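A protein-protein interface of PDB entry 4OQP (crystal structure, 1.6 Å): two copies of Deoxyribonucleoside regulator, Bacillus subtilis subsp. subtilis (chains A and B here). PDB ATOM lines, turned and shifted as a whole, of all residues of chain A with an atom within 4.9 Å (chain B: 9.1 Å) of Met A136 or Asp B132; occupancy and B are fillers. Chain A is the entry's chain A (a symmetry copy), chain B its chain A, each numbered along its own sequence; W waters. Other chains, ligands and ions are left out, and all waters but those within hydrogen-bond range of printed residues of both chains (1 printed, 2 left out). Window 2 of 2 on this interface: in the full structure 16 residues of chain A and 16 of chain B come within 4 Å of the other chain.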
ATOM      1  N   ASP A 132      -2.968 -15.399   3.069  1.00  0.00           N
ATOM      2  CA  ASP A 132      -2.384 -15.059   4.371  1.00  0.00           C
ATOM      3  C   ASP A 132      -3.046 -13.818   4.942  1.00  0.00           C
ATOM      4  O   ASP A 132      -3.438 -13.808   6.103  1.00  0.00           O
ATOM      5  CB  ASP A 132      -0.874 -14.879   4.286  1.00  0.00           C
ATOM      6  CG  ASP A 132      -0.140 -16.194   4.102  1.00  0.00           C
ATOM      7  OD1 ASP A 132      -0.624 -17.284   4.510  1.00  0.00           O
ATOM      8  OD2 ASP A 132       0.962 -16.119   3.558  1.00  0.00           O
ATOM      9  N   VAL A 133      -3.221 -12.790   4.115  1.00  0.00           N
ATOM     10  CA  VAL A 133      -3.901 -11.580   4.594  1.00  0.00           C
ATOM     11  C   VAL A 133      -5.365 -11.896   4.915  1.00  0.00           C
ATOM     12  O   VAL A 133      -5.887 -11.425   5.916  1.00  0.00           O
ATOM     13  CB  VAL A 133      -3.668 -10.343   3.685  1.00  0.00           C
ATOM     14  CG1 VAL A 133      -4.266 -10.513   2.296  1.00  0.00           C
ATOM     15  CG2 VAL A 133      -4.143  -9.049   4.367  1.00  0.00           C
ATOM     16  N   LYS A 134      -5.998 -12.720   4.091  1.00  0.00           N
ATOM     17  CA  LYS A 134      -7.379 -13.089   4.333  1.00  0.00           C
ATOM     18  C   LYS A 134      -7.516 -13.749   5.702  1.00  0.00           C
ATOM     19  O   LYS A 134      -8.420 -13.420   6.486  1.00  0.00           O
ATOM     20  CB  LYS A 134      -7.849 -14.033   3.216  1.00  0.00           C
ATOM     21  CG  LYS A 134      -9.257 -14.583   3.323  1.00  0.00           C
ATOM     22  CD  LYS A 134      -9.424 -15.789   4.207  1.00  0.00           C
ATOM     23  CE  LYS A 134     -10.708 -16.501   3.826  1.00  0.00           C
ATOM     24  NZ  LYS A 134     -10.996 -17.720   4.603  1.00  0.00           N
ATOM     25  N   ARG A 135      -6.627 -14.683   5.979  1.00  0.00           N
ATOM     26  CA  ARG A 135      -6.702 -15.396   7.255  1.00  0.00           C
ATOM     27  C   ARG A 135      -6.443 -14.464   8.424  1.00  0.00           C
ATOM     28  O   ARG A 135      -7.036 -14.651   9.479  1.00  0.00           O
ATOM     29  CB  ARG A 135      -5.770 -16.607   7.325  1.00  0.00           C
ATOM     30  CG  ARG A 135      -4.309 -16.301   7.134  1.00  0.00           C
ATOM     31  CD  ARG A 135      -3.412 -17.443   7.572  1.00  0.00           C
ATOM     32  NE  ARG A 135      -2.053 -16.960   7.794  1.00  0.00           N
ATOM     33  CZ  ARG A 135      -1.653 -16.362   8.909  1.00  0.00           C
ATOM     34  NH1 ARG A 135      -2.508 -16.184   9.908  1.00  0.00           N
ATOM     35  NH2 ARG A 135      -0.398 -15.937   9.014  1.00  0.00           N
ATOM     36  N   MET A 136      -5.564 -13.474   8.262  1.00  0.00           N
ATOM     37  CA  MET A 136      -5.289 -12.554   9.371  1.00  0.00           C
ATOM     38  C   MET A 136      -6.447 -11.574   9.571  1.00  0.00           C
ATOM     39  O   MET A 136      -6.790 -11.253  10.687  1.00  0.00           O
ATOM     40  CB  MET A 136      -3.960 -11.814   9.177  1.00  0.00           C
ATOM     41  CG  MET A 136      -2.757 -12.722   9.358  1.00  0.00           C
ATOM     42  SD  MET A 136      -2.654 -13.416  11.023  1.00  0.00           S
ATOM     43  CE  MET A 136      -2.126 -12.026  12.033  1.00  0.00           C
ATOM     44  N   VAL A 137      -7.043 -11.103   8.481  1.00  0.00           N
ATOM     45  CA  VAL A 137      -8.164 -10.188   8.559  1.00  0.00           C
ATOM     46  C   VAL A 137      -9.422 -10.824   9.170  1.00  0.00           C
ATOM     47  O   VAL A 137     -10.118 -10.179   9.985  1.00  0.00           O
ATOM     48  CB  VAL A 137      -8.483  -9.604   7.164  1.00  0.00           C
ATOM     49  CG1 VAL A 137      -9.867  -8.942   7.165  1.00  0.00           C
ATOM     50  CG2 VAL A 137      -7.360  -8.684   6.718  1.00  0.00           C
ATOM     51  N   GLU A 138      -9.709 -12.074   8.795  1.00  0.00           N
ATOM     52  CA  GLU A 138     -10.918 -12.751   9.242  1.00  0.00           C
ATOM     53  C   GLU A 138     -10.945 -13.071  10.718  1.00  0.00           C
ATOM     54  O   GLU A 138     -12.017 -13.366  11.256  1.00  0.00           O
ATOM     55  CB  GLU A 138     -11.192 -14.003   8.414  1.00  0.00           C
ATOM     56  CG  GLU A 138     -10.287 -15.169   8.771  1.00  0.00           C
ATOM     57  CD  GLU A 138     -10.503 -16.358   7.882  1.00  0.00           C
ATOM     58  OE1 GLU A 138     -11.568 -16.401   7.157  1.00  0.00           O
ATOM     59  OE2 GLU A 138      -9.642 -17.304   7.909  1.00  0.00           O
ATOM     60  N   LYS A 139      -9.773 -13.075  11.370  1.00  0.00           N
ATOM     61  CA  LYS A 139      -9.663 -13.336  12.805  1.00  0.00           C
ATOM     62  C   LYS A 139     -10.089 -12.159  13.684  1.00  0.00           C
ATOM     63  O   LYS A 139     -10.232 -12.327  14.876  1.00  0.00           O
ATOM     64  CB  LYS A 139      -8.226 -13.732  13.160  1.00  0.00           C
ATOM     65  CG  LYS A 139      -7.778 -15.087  12.643  1.00  0.00           C
ATOM     66  CD  LYS A 139      -6.289 -15.242  12.959  1.00  0.00           C
ATOM     67  CE  LYS A 139      -5.729 -16.602  12.564  1.00  0.00           C
ATOM     68  NZ  LYS A 139      -5.547 -17.482  13.747  1.00  0.00           N
ATOM     69  N   ASP A 140     -10.249 -10.970  13.124  1.00  0.00           N
ATOM     70  CA  ASP A 140     -10.767  -9.820  13.885  1.00  0.00           C
ATOM     71  C   ASP A 140     -12.146 -10.184  14.442  1.00  0.00           C
ATOM     72  O   ASP A 140     -13.020 -10.653  13.688  1.00  0.00           O
ATOM     73  CB  ASP A 140     -10.845  -8.585  12.956  1.00  0.00           C
ATOM     74  CG  ASP A 140     -11.392  -7.361  13.598  1.00  0.00           C
ATOM     75  OD1 ASP A 140     -12.556  -7.361  14.074  1.00  0.00           O
ATOM     76  OD2 ASP A 140     -10.678  -6.311  13.647  1.00  0.00           O
ATOM     77  N   PHE B 128      -5.614  -1.408  13.309  1.00  0.00           N
ATOM     78  CA  PHE B 128      -5.796  -2.853  13.175  1.00  0.00           C
ATOM     79  C   PHE B 128      -5.482  -3.578  14.486  1.00  0.00           C
ATOM     80  O   PHE B 128      -4.887  -3.011  15.379  1.00  0.00           O
ATOM     81  CB  PHE B 128      -4.903  -3.395  12.047  1.00  0.00           C
ATOM     82  CG  PHE B 128      -5.312  -2.881  10.696  1.00  0.00           C
ATOM     83  CD1 PHE B 128      -5.028  -1.594  10.325  1.00  0.00           C
ATOM     84  CD2 PHE B 128      -6.078  -3.668   9.856  1.00  0.00           C
ATOM     85  CE1 PHE B 128      -5.475  -1.097   9.118  1.00  0.00           C
ATOM     86  CE2 PHE B 128      -6.541  -3.153   8.658  1.00  0.00           C
ATOM     87  CZ  PHE B 128      -6.213  -1.889   8.285  1.00  0.00           C
ATOM     88  N   ASP B 129      -5.945  -4.827  14.592  1.00  0.00           N
ATOM     89  CA  ASP B 129      -5.786  -5.583  15.832  1.00  0.00           C
ATOM     90  C   ASP B 129      -4.326  -5.880  16.198  1.00  0.00           C
ATOM     91  O   ASP B 129      -4.005  -6.051  17.381  1.00  0.00           O
ATOM     92  CB  ASP B 129      -6.485  -6.928  15.753  1.00  0.00           C
ATOM     93  CG  ASP B 129      -7.932  -6.858  16.039  1.00  0.00           C
ATOM     94  OD1 ASP B 129      -8.475  -5.799  16.467  1.00  0.00           O
ATOM     95  OD2 ASP B 129      -8.545  -7.922  15.828  1.00  0.00           O
ATOM     96  N   ASN B 130      -3.461  -5.984  15.201  1.00  0.00           N
ATOM     97  CA  ASN B 130      -2.072  -6.356  15.444  1.00  0.00           C
ATOM     98  C   ASN B 130      -1.204  -5.907  14.276  1.00  0.00           C
ATOM     99  O   ASN B 130      -1.719  -5.542  13.199  1.00  0.00           O
ATOM    100  CB  ASN B 130      -1.926  -7.859  15.722  1.00  0.00           C
ATOM    101  CG  ASN B 130      -2.307  -8.690  14.538  1.00  0.00           C
ATOM    102  OD1 ASN B 130      -1.628  -8.665  13.504  1.00  0.00           O
ATOM    103  ND2 ASN B 130      -3.457  -9.331  14.613  1.00  0.00           N
ATOM    104  N   ALA B 131       0.103  -5.857  14.507  1.00  0.00           N
ATOM    105  CA  ALA B 131       1.029  -5.266  13.508  1.00  0.00           C
ATOM    106  C   ALA B 131       1.210  -6.192  12.301  1.00  0.00           C
ATOM    107  O   ALA B 131       1.555  -5.726  11.208  1.00  0.00           O
ATOM    108  CB  ALA B 131       2.376  -4.992  14.152  1.00  0.00           C
ATOM    109  N   ASP B 132       0.966  -7.492  12.502  1.00  0.00           N
ATOM    110  CA  ASP B 132       1.135  -8.456  11.410  1.00  0.00           C
ATOM    111  C   ASP B 132       0.060  -8.257  10.355  1.00  0.00           C
ATOM    112  O   ASP B 132       0.365  -8.194   9.170  1.00  0.00           O
ATOM    113  CB  ASP B 132       1.140  -9.892  11.915  1.00  0.00           C
ATOM    114  CG  ASP B 132       2.415 -10.244  12.658  1.00  0.00           C
ATOM    115  OD1 ASP B 132       3.503  -9.655  12.418  1.00  0.00           O
ATOM    116  OD2 ASP B 132       2.320 -11.154  13.482  1.00  0.00           O
ATOM    117  N   VAL B 133      -1.189  -8.103  10.786  1.00  0.00           N
ATOM    118  CA  VAL B 133      -2.266  -7.857   9.819  1.00  0.00           C
ATOM    119  C   VAL B 133      -2.063  -6.495   9.148  1.00  0.00           C
ATOM    120  O   VAL B 133      -2.260  -6.371   7.947  1.00  0.00           O
ATOM    121  CB  VAL B 133      -3.684  -8.111  10.399  1.00  0.00           C
ATOM    122  CG1 VAL B 133      -4.042  -7.149  11.522  1.00  0.00           C
ATOM    123  CG2 VAL B 133      -4.749  -8.129   9.288  1.00  0.00           C
ATOM    124  N   LYS B 134      -1.633  -5.504   9.915  1.00  0.00           N
ATOM    125  CA  LYS B 134      -1.394  -4.187   9.355  1.00  0.00           C
ATOM    126  C   LYS B 134      -0.360  -4.271   8.236  1.00  0.00           C
ATOM    127  O   LYS B 134      -0.543  -3.699   7.150  1.00  0.00           O
ATOM    128  CB  LYS B 134      -0.921  -3.245  10.474  1.00  0.00           C
ATOM    129  CG  LYS B 134      -0.558  -1.829  10.076  1.00  0.00           C
ATOM    130  CD  LYS B 134       0.831  -1.636   9.532  1.00  0.00           C
ATOM    131  CE  LYS B 134       1.209  -0.173   9.661  1.00  0.00           C
ATOM    132  NZ  LYS B 134       2.562   0.164   9.179  1.00  0.00           N
ATOM    133  N   ARG B 135       0.723  -4.972   8.507  1.00  0.00           N
ATOM    134  CA  ARG B 135       1.784  -5.077   7.505  1.00  0.00           C
ATOM    135  C   ARG B 135       1.312  -5.831   6.277  1.00  0.00           C
ATOM    136  O   ARG B 135       1.741  -5.509   5.176  1.00  0.00           O
ATOM    137  CB  ARG B 135       3.069  -5.704   8.051  1.00  0.00           C
ATOM    138  CG  ARG B 135       2.916  -7.095   8.606  1.00  0.00           C
ATOM    139  CD  ARG B 135       4.246  -7.800   8.788  1.00  0.00           C
ATOM    140  NE  ARG B 135       4.044  -9.241   8.887  1.00  0.00           N
ATOM    141  CZ  ARG B 135       3.886 -10.041   7.840  1.00  0.00           C
ATOM    142  NH1 ARG B 135       3.919  -9.538   6.612  1.00  0.00           N
ATOM    143  NH2 ARG B 135       3.687 -11.341   8.028  1.00  0.00           N
ATOM    144  N   MET B 136       0.447  -6.834   6.443  1.00  0.00           N
ATOM    145  CA  MET B 136      -0.031  -7.585   5.278  1.00  0.00           C
ATOM    146  C   MET B 136      -1.044  -6.766   4.474  1.00  0.00           C
ATOM    147  O   MET B 136      -1.039  -6.805   3.265  1.00  0.00           O
ATOM    148  CB  MET B 136      -0.610  -8.947   5.681  1.00  0.00           C
ATOM    149  CG  MET B 136       0.460  -9.924   6.132  1.00  0.00           C
ATOM    150  SD  MET B 136       1.650 -10.303   4.826  1.00  0.00           S
ATOM    151  CE  MET B 136       0.733 -11.369   3.708  1.00  0.00           C
ATOM    152  N   VAL B 137      -1.908  -6.025   5.159  1.00  0.00           N
ATOM    153  CA  VAL B 137      -2.893  -5.195   4.495  1.00  0.00           C
ATOM    154  C   VAL B 137      -2.270  -4.031   3.707  1.00  0.00           C
ATOM    155  O   VAL B 137      -2.713  -3.733   2.575  1.00  0.00           O
ATOM    156  CB  VAL B 137      -3.924  -4.659   5.515  1.00  0.00           C
ATOM    157  CG1 VAL B 137      -4.730  -3.505   4.905  1.00  0.00           C
ATOM    158  CG2 VAL B 137      -4.779  -5.801   6.035  1.00  0.00           C
ATOM    159  N   GLU B 138      -1.253  -3.387   4.285  1.00  0.00           N
ATOM    160  CA  GLU B 138      -0.637  -2.218   3.674  1.00  0.00           C
ATOM    161  C   GLU B 138       0.125  -2.509   2.402  1.00  0.00           C
ATOM    162  O   GLU B 138       0.429  -1.576   1.650  1.00  0.00           O
ATOM    163  CB  GLU B 138       0.242  -1.468   4.670  1.00  0.00           C
ATOM    164  CG  GLU B 138       1.571  -2.154   4.934  1.00  0.00           C
ATOM    165  CD  GLU B 138       2.380  -1.457   5.988  1.00  0.00           C
ATOM    166  OE1 GLU B 138       2.050  -0.257   6.325  1.00  0.00           O
ATOM    167  OE2 GLU B 138       3.392  -2.064   6.482  1.00  0.00           O
ATOM    168  N   LYS B 139       0.491  -3.779   2.177  1.00  0.00           N
ATOM    169  CA  LYS B 139       1.203  -4.199   0.971  1.00  0.00           C
ATOM    170  C   LYS B 139       0.317  -4.288  -0.273  1.00  0.00           C
ATOM    171  O   LYS B 139       0.831  -4.429  -1.362  1.00  0.00           O
ATOM    172  CB  LYS B 139       1.878  -5.556   1.203  1.00  0.00           C
ATOM    173  CG  LYS B 139       3.048  -5.542   2.170  1.00  0.00           C
ATOM    174  CD  LYS B 139       3.492  -6.990   2.392  1.00  0.00           C
ATOM    175  CE  LYS B 139       4.719  -7.112   3.283  1.00  0.00           C
ATOM    176  NZ  LYS B 139       5.944  -7.398   2.491  1.00  0.00           N
ATOM    177  N   ALA B 206       3.805   0.266  19.814  1.00  0.00           N
ATOM    178  CA  ALA B 206       2.981  -0.865  19.450  1.00  0.00           C
ATOM    179  C   ALA B 206       1.670  -0.443  18.781  1.00  0.00           C
ATOM    180  O   ALA B 206       1.294  -1.012  17.754  1.00  0.00           O
ATOM    181  CB  ALA B 206       2.678  -1.708  20.682  1.00  0.00           C
ATOM    182  N   ASP B 209       2.364   1.114  15.384  1.00  0.00           N
ATOM    183  CA  ASP B 209       2.711   0.074  14.400  1.00  0.00           C
ATOM    184  C   ASP B 209       1.496  -0.694  13.888  1.00  0.00           C
ATOM    185  O   ASP B 209       1.618  -1.469  12.940  1.00  0.00           O
ATOM    186  CB  ASP B 209       3.665  -0.955  15.015  1.00  0.00           C
ATOM    187  CG  ASP B 209       5.083  -0.462  15.132  1.00  0.00           C
ATOM    188  OD1 ASP B 209       5.423   0.626  14.625  1.00  0.00           O
ATOM    189  OD2 ASP B 209       5.881  -1.199  15.750  1.00  0.00           O
ATOM    190  N   ARG B 210       0.331  -0.491  14.525  1.00  0.00           N
ATOM    191  CA  ARG B 210      -0.964  -1.093  14.104  1.00  0.00           C
ATOM    192  C   ARG B 210      -1.820  -0.118  13.288  1.00  0.00           C
ATOM    193  O   ARG B 210      -2.913  -0.424  12.939  1.00  0.00           O
ATOM    194  CB  ARG B 210      -1.751  -1.542  15.356  1.00  0.00           C
ATOM    195  CG  ARG B 210      -1.137  -2.749  16.026  1.00  0.00           C
ATOM    196  CD  ARG B 210      -1.662  -2.899  17.440  1.00  0.00           C
ATOM    197  NE  ARG B 210      -3.108  -2.871  17.445  1.00  0.00           N
ATOM    198  CZ  ARG B 210      -3.864  -2.857  18.539  1.00  0.00           C
ATOM    199  NH1 ARG B 210      -3.319  -2.852  19.746  1.00  0.00           N
ATOM    200  NH2 ARG B 210      -5.196  -2.802  18.401  1.00  0.00           N
ATOM    201  N   THR B 211      -1.244   1.014  12.918  1.00  0.00           N
ATOM    202  CA  THR B 211      -2.006   2.111  12.351  1.00  0.00           C
ATOM    203  C   THR B 211      -1.588   2.344  10.908  1.00  0.00           C
ATOM    204  O   THR B 211      -0.362   2.425  10.581  1.00  0.00           O
ATOM    205  CB  THR B 211      -1.769   3.353  13.228  1.00  0.00           C
ATOM    206  OG1 THR B 211      -2.174   3.067  14.575  1.00  0.00           O
ATOM    207  CG2 THR B 211      -2.564   4.495  12.674  1.00  0.00           C
ATOM    208  N   ILE B 212      -2.579   2.417  10.011  1.00  0.00           N
ATOM    209  CA  ILE B 212      -2.307   2.766   8.612  1.00  0.00           C
ATOM    210  C   ILE B 212      -2.833   4.157   8.341  1.00  0.00           C
ATOM    211  O   ILE B 212      -4.014   4.397   8.505  1.00  0.00           O
ATOM    212  CB  ILE B 212      -2.892   1.760   7.620  1.00  0.00           C
ATOM    213  CG1 ILE B 212      -2.235   0.374   7.812  1.00  0.00           C
ATOM    214  CG2 ILE B 212      -2.802   2.266   6.169  1.00  0.00           C
ATOM    215  CD1 ILE B 212      -2.812  -0.698   6.918  1.00  0.00           C
HETATM  216  O   HOH W   1      -5.024 -11.275  12.942  1.00  0.00           O
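Water W1 bridges O of Met A136 (2.9 Å) and ND2 of Asn B130 (3.0 Å).
The side-chain carboxylate (OD2) of Asp A140 sits close to the side-chain carboxylate (OD2) of Asp B129, at 3.4 Å.
Printed residues of chain B within 4 Å of Met A136: Asn B130, Asp B132 and Val B133. Of the printed residues of chain A, Asp B132 touches Met A136 (3.9 Å). Of chain B, only Val B133 (3.7 Å) and Val B137 (3.9 Å) come within 4 Å of Val A137. Printed residues of chain A within 4 Å of Met B136: Asp A132 and Val A133. Of the printed residues of chain B, Asp A140 touches Asp B129 (3.4 Å). Arg A135 touches none of the printed residues of chain B. Phe B128 touches none of the printed residues of chain A. The nearest printed residue of chain A that does not touch Asp B132 is Val A133 (6.6 Å).
Printed residues of chain A that touch a printed residue of chain B: Asp A132, Val A133, Met A136, Val A137 and Asp A140. Along chain A the printed residues that touch a printed residue of chain B span positions 132 to 140. Printed residues of chain B that touch a printed residue of chain A: Asp B129, Asn B130, Asp B132, Val B133, Met B136 and Val B137. Among the printed residues, no Asp or Glu carboxylate lies within 4 Å of a Lys or Arg side-chain nitrogen of the other chain.
The backbone NH of Asp B132 is in hydrogen-bond range of the side-chain amide oxygen of Asn B130, 3.0 Å away. OD1 of Asn B130 is in hydrogen-bond range of N of Val B133, at 2.8 Å. The guanidinium group of Arg B135 lies within salt-bridge range of the side-chain carboxylate of Asp B132 (3.6 Å). The guanidinium group (NH1) of Arg B135 sits at hydrogen-bond distance from the side-chain sulfur (SD) of Met B136 (3.0 Å). NE of Arg A135 is in salt-bridge range of OD1 of Asp A132 (3.6 Å). The side-chain sulfur of Met A136 is in hydrogen-bond range of the guanidinium group of Arg A135 (3.0 Å).
Asp A132 touches Met B136, and with the chains exchanged Met A136 touches Asp B132. Val A133 touches Met B136, and with the chains exchanged Met A136 touches Val B133. Val A133 touches Val B137, and with the chains exchanged Val A137 touches Val B133. Val A137 touches its own counterpart, Val B137.
Among the printed residues, pairs that only touch across the chains: Asp A132 with Met B136, Val A133 with Met B136, Val A133 with Val B137, Met A136 with Asn B130, Met A136 with Asp B132, Met A136 with Val B133, Val A137 with Val B133 and Val A137 with Val B137.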
